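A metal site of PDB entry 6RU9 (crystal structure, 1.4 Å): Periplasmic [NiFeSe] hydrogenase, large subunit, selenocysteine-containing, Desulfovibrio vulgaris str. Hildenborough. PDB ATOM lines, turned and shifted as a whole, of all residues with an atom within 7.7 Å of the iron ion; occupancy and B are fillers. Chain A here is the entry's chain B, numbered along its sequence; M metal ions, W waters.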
ATOM      1  N   GLU A  53     -17.365 -15.992 -22.909  1.00  0.00           N
ATOM      2  CA  GLU A  53     -16.190 -15.814 -23.737  1.00  0.00           C
ATOM      3  C   GLU A  53     -15.579 -17.140 -24.161  1.00  0.00           C
ATOM      4  O   GLU A  53     -14.941 -17.197 -25.224  1.00  0.00           O
ATOM      5  CB  GLU A  53     -15.187 -14.907 -23.027  1.00  0.00           C
ATOM      6  CG  GLU A  53     -15.766 -13.481 -22.869  1.00  0.00           C
ATOM      7  CD  GLU A  53     -15.197 -12.674 -21.688  1.00  0.00           C
ATOM      8  OE1 GLU A  53     -14.813 -13.267 -20.675  1.00  0.00           O
ATOM      9  OE2 GLU A  53     -15.139 -11.420 -21.779  1.00  0.00           O
ATOM     10  N   GLU A 279      -7.608  -5.302 -17.895  1.00  0.00           N
ATOM     11  CA  GLU A 279      -8.441  -6.022 -16.921  1.00  0.00           C
ATOM     12  C   GLU A 279      -7.556  -6.803 -15.960  1.00  0.00           C
ATOM     13  O   GLU A 279      -6.809  -7.698 -16.370  1.00  0.00           O
ATOM     14  CB  GLU A 279      -9.432  -6.957 -17.630  1.00  0.00           C
ATOM     15  CG  GLU A 279     -10.455  -6.227 -18.409  1.00  0.00           C
ATOM     16  CD  GLU A 279     -11.587  -7.124 -18.855  1.00  0.00           C
ATOM     17  OE1 GLU A 279     -11.431  -7.751 -19.924  1.00  0.00           O
ATOM     18  OE2 GLU A 279     -12.615  -7.199 -18.137  1.00  0.00           O
ATOM     19  N   PHE A 286      -9.985 -15.826 -11.505  1.00  0.00           N
ATOM     20  CA  PHE A 286      -9.387 -16.150 -12.787  1.00  0.00           C
ATOM     21  C   PHE A 286      -7.901 -16.389 -12.589  1.00  0.00           C
ATOM     22  O   PHE A 286      -7.291 -15.892 -11.637  1.00  0.00           O
ATOM     23  CB  PHE A 286      -9.638 -15.054 -13.834  1.00  0.00           C
ATOM     24  CG  PHE A 286     -11.089 -14.813 -14.063  1.00  0.00           C
ATOM     25  CD1 PHE A 286     -11.810 -15.678 -14.865  1.00  0.00           C
ATOM     26  CD2 PHE A 286     -11.778 -13.824 -13.370  1.00  0.00           C
ATOM     27  CE1 PHE A 286     -13.156 -15.530 -15.047  1.00  0.00           C
ATOM     28  CE2 PHE A 286     -13.143 -13.663 -13.546  1.00  0.00           C
ATOM     29  CZ  PHE A 286     -13.837 -14.517 -14.371  1.00  0.00           C
ATOM     30  N   TYR A 295      -8.398  -5.961 -23.816  1.00  0.00           N
ATOM     31  CA  TYR A 295      -9.416  -6.886 -24.311  1.00  0.00           C
ATOM     32  C   TYR A 295      -9.000  -7.543 -25.635  1.00  0.00           C
ATOM     33  O   TYR A 295      -9.439  -8.665 -25.923  1.00  0.00           O
ATOM     34  CB  TYR A 295     -10.780  -6.176 -24.444  1.00  0.00           C
ATOM     35  CG  TYR A 295     -10.688  -4.979 -25.355  1.00  0.00           C
ATOM     36  CD1 TYR A 295     -10.802  -5.128 -26.742  1.00  0.00           C
ATOM     37  CD2 TYR A 295     -10.422  -3.704 -24.855  1.00  0.00           C
ATOM     38  CE1 TYR A 295     -10.677  -4.054 -27.591  1.00  0.00           C
ATOM     39  CE2 TYR A 295     -10.273  -2.621 -25.715  1.00  0.00           C
ATOM     40  CZ  TYR A 295     -10.431  -2.798 -27.078  1.00  0.00           C
ATOM     41  OH  TYR A 295     -10.291  -1.742 -27.944  1.00  0.00           O
ATOM     42  N   LYS A 299      -8.183 -12.997 -21.999  1.00  0.00           N
ATOM     43  CA  LYS A 299      -8.290 -14.429 -21.751  1.00  0.00           C
ATOM     44  C   LYS A 299      -9.215 -14.612 -20.564  1.00  0.00           C
ATOM     45  O   LYS A 299      -9.263 -13.759 -19.650  1.00  0.00           O
ATOM     46  CB  LYS A 299      -6.930 -15.056 -21.432  1.00  0.00           C
ATOM     47  CG  LYS A 299      -5.973 -15.065 -22.595  1.00  0.00           C
ATOM     48  CD  LYS A 299      -4.610 -15.563 -22.135  1.00  0.00           C
ATOM     49  CE  LYS A 299      -3.678 -15.846 -23.302  1.00  0.00           C
ATOM     50  NZ  LYS A 299      -4.182 -16.979 -24.143  1.00  0.00           N
ATOM     51  N   THR A 300      -9.957 -15.710 -20.571  1.00  0.00           N
ATOM     52  CA  THR A 300     -10.901 -16.027 -19.510  1.00  0.00           C
ATOM     53  C   THR A 300     -10.709 -17.462 -19.067  1.00  0.00           C
ATOM     54  O   THR A 300     -11.174 -18.385 -19.737  1.00  0.00           O
ATOM     55  CB  THR A 300     -12.321 -15.741 -19.999  1.00  0.00           C
ATOM     56  OG1 THR A 300     -12.366 -14.374 -20.442  1.00  0.00           O
ATOM     57  CG2 THR A 300     -13.298 -15.982 -18.878  1.00  0.00           C
ATOM     58  N   PHE A 312     -16.273 -12.993  -9.371  1.00  0.00           N
ATOM     59  CA  PHE A 312     -16.147 -13.386 -10.765  1.00  0.00           C
ATOM     60  C   PHE A 312     -16.076 -12.200 -11.727  1.00  0.00           C
ATOM     61  O   PHE A 312     -15.953 -12.401 -12.944  1.00  0.00           O
ATOM     62  CB  PHE A 312     -17.278 -14.325 -11.193  1.00  0.00           C
ATOM     63  CG  PHE A 312     -17.152 -15.729 -10.643  1.00  0.00           C
ATOM     64  CD1 PHE A 312     -16.104 -16.556 -11.009  1.00  0.00           C
ATOM     65  CD2 PHE A 312     -18.082 -16.200  -9.740  1.00  0.00           C
ATOM     66  CE1 PHE A 312     -16.013 -17.846 -10.501  1.00  0.00           C
ATOM     67  CE2 PHE A 312     -17.990 -17.478  -9.220  1.00  0.00           C
ATOM     68  CZ  PHE A 312     -16.980 -18.312  -9.600  1.00  0.00           C
ATOM     69  N   LYS A 314     -14.008  -9.280 -13.321  1.00  0.00           N
ATOM     70  CA  LYS A 314     -12.642  -8.801 -13.484  1.00  0.00           C
ATOM     71  C   LYS A 314     -12.571  -7.321 -13.082  1.00  0.00           C
ATOM     72  O   LYS A 314     -13.589  -6.663 -12.871  1.00  0.00           O
ATOM     73  CB  LYS A 314     -12.176  -8.951 -14.932  1.00  0.00           C
ATOM     74  CG  LYS A 314     -12.056 -10.398 -15.447  1.00  0.00           C
ATOM     75  CD  LYS A 314     -11.527 -10.433 -16.893  1.00  0.00           C
ATOM     76  CE  LYS A 314     -11.488 -11.841 -17.485  1.00  0.00           C
ATOM     77  NZ  LYS A 314     -11.329 -11.833 -18.987  1.00  0.00           N
ATOM     78  N   LEU A 423     -18.215  -2.799 -24.684  1.00  0.00           N
ATOM     79  CA  LEU A 423     -17.482  -3.149 -25.893  1.00  0.00           C
ATOM     80  C   LEU A 423     -17.403  -4.649 -26.024  1.00  0.00           C
ATOM     81  O   LEU A 423     -17.298  -5.375 -25.033  1.00  0.00           O
ATOM     82  CB  LEU A 423     -16.083  -2.519 -25.924  1.00  0.00           C
ATOM     83  CG  LEU A 423     -15.035  -3.145 -25.031  1.00  0.00           C
ATOM     84  CD1 LEU A 423     -14.342  -4.317 -25.729  1.00  0.00           C
ATOM     85  CD2 LEU A 423     -14.017  -2.072 -24.648  1.00  0.00           C
ATOM     86  N   TYR A 436     -13.395 -13.982 -28.246  1.00  0.00           N
ATOM     87  CA  TYR A 436     -14.484 -13.008 -28.102  1.00  0.00           C
ATOM     88  C   TYR A 436     -14.367 -12.485 -26.677  1.00  0.00           C
ATOM     89  O   TYR A 436     -14.335 -13.289 -25.739  1.00  0.00           O
ATOM     90  CB  TYR A 436     -15.843 -13.667 -28.356  1.00  0.00           C
ATOM     91  CG  TYR A 436     -16.972 -12.690 -28.691  1.00  0.00           C
ATOM     92  CD1 TYR A 436     -17.504 -11.838 -27.727  1.00  0.00           C
ATOM     93  CD2 TYR A 436     -17.495 -12.618 -29.971  1.00  0.00           C
ATOM     94  CE1 TYR A 436     -18.546 -10.942 -28.041  1.00  0.00           C
ATOM     95  CE2 TYR A 436     -18.496 -11.738 -30.315  1.00  0.00           C
ATOM     96  CZ  TYR A 436     -19.026 -10.897 -29.341  1.00  0.00           C
ATOM     97  OH  TYR A 436     -20.024 -10.038 -29.696  1.00  0.00           O
ATOM     98  N   GLN A 437     -14.229 -11.184 -26.514  1.00  0.00           N
ATOM     99  CA  GLN A 437     -14.032 -10.566 -25.201  1.00  0.00           C
ATOM    100  C   GLN A 437     -15.045  -9.449 -25.028  1.00  0.00           C
ATOM    101  O   GLN A 437     -15.266  -8.649 -25.923  1.00  0.00           O
ATOM    102  CB  GLN A 437     -12.599 -10.043 -25.040  1.00  0.00           C
ATOM    103  CG  GLN A 437     -11.583 -11.175 -24.864  1.00  0.00           C
ATOM    104  CD  GLN A 437     -11.717 -11.892 -23.560  1.00  0.00           C
ATOM    105  OE1 GLN A 437     -11.855 -11.280 -22.519  1.00  0.00           O
ATOM    106  NE2 GLN A 437     -11.640 -13.214 -23.590  1.00  0.00           N
ATOM    107  N   ILE A 438     -15.643  -9.424 -23.849  1.00  0.00           N
ATOM    108  CA  ILE A 438     -16.680  -8.481 -23.468  1.00  0.00           C
ATOM    109  C   ILE A 438     -16.172  -7.669 -22.286  1.00  0.00           C
ATOM    110  O   ILE A 438     -15.692  -8.220 -21.300  1.00  0.00           O
ATOM    111  CB  ILE A 438     -18.008  -9.196 -23.124  1.00  0.00           C
ATOM    112  CG1 ILE A 438     -18.558  -9.878 -24.382  1.00  0.00           C
ATOM    113  CG2 ILE A 438     -19.011  -8.218 -22.538  1.00  0.00           C
ATOM    114  CD1 ILE A 438     -19.026 -11.239 -24.153  1.00  0.00           C
ATOM    115  N   VAL A 439     -16.303  -6.355 -22.381  1.00  0.00           N
ATOM    116  CA  VAL A 439     -15.995  -5.437 -21.288  1.00  0.00           C
ATOM    117  C   VAL A 439     -17.261  -4.594 -21.131  1.00  0.00           C
ATOM    118  O   VAL A 439     -17.549  -3.745 -21.970  1.00  0.00           O
ATOM    119  CB  VAL A 439     -14.782  -4.553 -21.621  1.00  0.00           C
ATOM    120  CG1 VAL A 439     -14.504  -3.602 -20.460  1.00  0.00           C
ATOM    121  CG2 VAL A 439     -13.532  -5.410 -21.933  1.00  0.00           C
ATOM    122  N   SER A 440     -18.050  -4.856 -20.086  1.00  0.00           N
ATOM    123  CA  SER A 440     -19.418  -4.387 -19.979  1.00  0.00           C
ATOM    124  C   SER A 440     -19.567  -3.309 -18.917  1.00  0.00           C
ATOM    125  O   SER A 440     -18.617  -2.960 -18.194  1.00  0.00           O
ATOM    126  CB  SER A 440     -20.314  -5.579 -19.623  1.00  0.00           C
ATOM    127  OG  SER A 440     -19.857  -5.997 -18.367  1.00  0.00           O
ATOM    128  N   LEU A 443     -19.373  -4.260 -15.196  1.00  0.00           N
ATOM    129  CA  LEU A 443     -17.968  -4.576 -14.969  1.00  0.00           C
ATOM    130  C   LEU A 443     -17.195  -3.355 -14.516  1.00  0.00           C
ATOM    131  O   LEU A 443     -16.414  -3.417 -13.562  1.00  0.00           O
ATOM    132  CB  LEU A 443     -17.408  -5.169 -16.259  1.00  0.00           C
ATOM    133  CG  LEU A 443     -15.888  -5.264 -16.353  1.00  0.00           C
ATOM    134  CD1 LEU A 443     -15.327  -6.331 -15.454  1.00  0.00           C
ATOM    135  CD2 LEU A 443     -15.514  -5.552 -17.791  1.00  0.00           C
ATOM    136  N   CYS A 489     -24.342  -9.036 -16.629  1.00  0.00           N
ATOM    137  CA  CYS A 489     -23.453  -8.275 -17.496  1.00  0.00           C
ATOM    138  C   CYS A 489     -22.030  -8.230 -16.952  1.00  0.00           C
ATOM    139  O   CYS A 489     -21.063  -8.369 -17.711  1.00  0.00           O
ATOM    140  CB  CYS A 489     -23.983  -6.833 -17.670  1.00  0.00           C
ATOM    141  SG  CYS A 489     -25.237  -6.749 -18.875  1.00  0.00           S
ATOM    142  N   ALA A 490     -21.873  -7.936 -15.663  1.00  0.00           N
ATOM    143  CA  ALA A 490     -20.521  -7.737 -15.117  1.00  0.00           C
ATOM    144  C   ALA A 490     -19.643  -8.979 -15.305  1.00  0.00           C
ATOM    145  O   ALA A 490     -18.437  -8.849 -15.577  1.00  0.00           O
ATOM    146  CB  ALA A 490     -20.582  -7.354 -13.638  1.00  0.00           C
ATOM    147  N   VAL A 491     -20.212 -10.179 -15.126  1.00  0.00           N
ATOM    148  CA  VAL A 491     -19.440 -11.425 -15.117  1.00  0.00           C
ATOM    149  C   VAL A 491     -19.440 -12.092 -16.496  1.00  0.00           C
ATOM    150  O   VAL A 491     -18.417 -12.607 -16.955  1.00  0.00           O
ATOM    151  CB  VAL A 491     -19.968 -12.390 -14.043  1.00  0.00           C
ATOM    152  CG1 VAL A 491     -19.208 -13.701 -14.140  1.00  0.00           C
ATOM    153  CG2 VAL A 491     -19.904 -11.825 -12.621  1.00  0.00           C
ATOM    154  N   HIS A 492     -20.628 -12.190 -17.104  1.00  0.00           N
ATOM    155  CA  HIS A 492     -20.831 -12.917 -18.366  1.00  0.00           C
ATOM    156  C   HIS A 492     -20.207 -14.312 -18.283  1.00  0.00           C
ATOM    157  O   HIS A 492     -20.407 -15.051 -17.300  1.00  0.00           O
ATOM    158  CB  HIS A 492     -20.462 -12.106 -19.603  1.00  0.00           C
ATOM    159  CG  HIS A 492     -19.210 -11.294 -19.496  1.00  0.00           C
ATOM    160  ND1 HIS A 492     -19.164 -10.074 -18.842  1.00  0.00           N
ATOM    161  CD2 HIS A 492     -17.966 -11.506 -19.980  1.00  0.00           C
ATOM    162  CE1 HIS A 492     -17.939  -9.588 -18.914  1.00  0.00           C
ATOM    163  NE2 HIS A 492     -17.190 -10.440 -19.594  1.00  0.00           N
ATOM    164  OXT HIS A 492     -19.484 -14.708 -19.224  1.00  0.00           O
HETATM  165 FE    FE M   1     -15.103 -10.001 -20.049  1.00  0.00          FE
HETATM  166  O   HOH W   1     -14.444 -11.701 -18.682  1.00  0.00           O
HETATM  167  O   HOH W   2     -14.759  -8.710 -18.335  1.00  0.00           O
HETATM  168  O   HOH W   3     -13.000  -9.730 -20.526  1.00  0.00           O
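Three residues have an atom within 4 Å of the iron ion: Glu 53, Ile 438 and His 492. The nearest printed residue that does not touch the iron ion is Glu 279 (4.2 Å).
ND1 of His 492 lies within hydrogen-bond range of O of Cys 489, 2.8 Å away. OE2 of Glu 53 sits close to OE1 of Gln 437 (3.4 Å). The side-chain carboxylate of Glu 53 is in hydrogen-bond range of the side-chain hydroxyl of Thr 300, at 2.7 Å.
Water W1 lies within hydrogen-bond range of OE1 of Glu 53 (2.6 Å) and NZ of Lys 314 (3.1 Å). Water W3 lies within hydrogen-bond range of OE1 of Glu 279 (2.6 Å), OE1 of Gln 437 (2.8 Å) and NZ of Lys 314 (3.1 Å).
The iron ion is bound by water W3 (2.2 Å), water W2 (2.2 Å), a ring nitrogen (NE2) of His 492 (2.2 Å), the side-chain carboxylate of Glu 53 (2.2 Å), the backbone carbonyl oxygen of Ile 438 (2.3 Å) and water W1 (2.3 Å).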
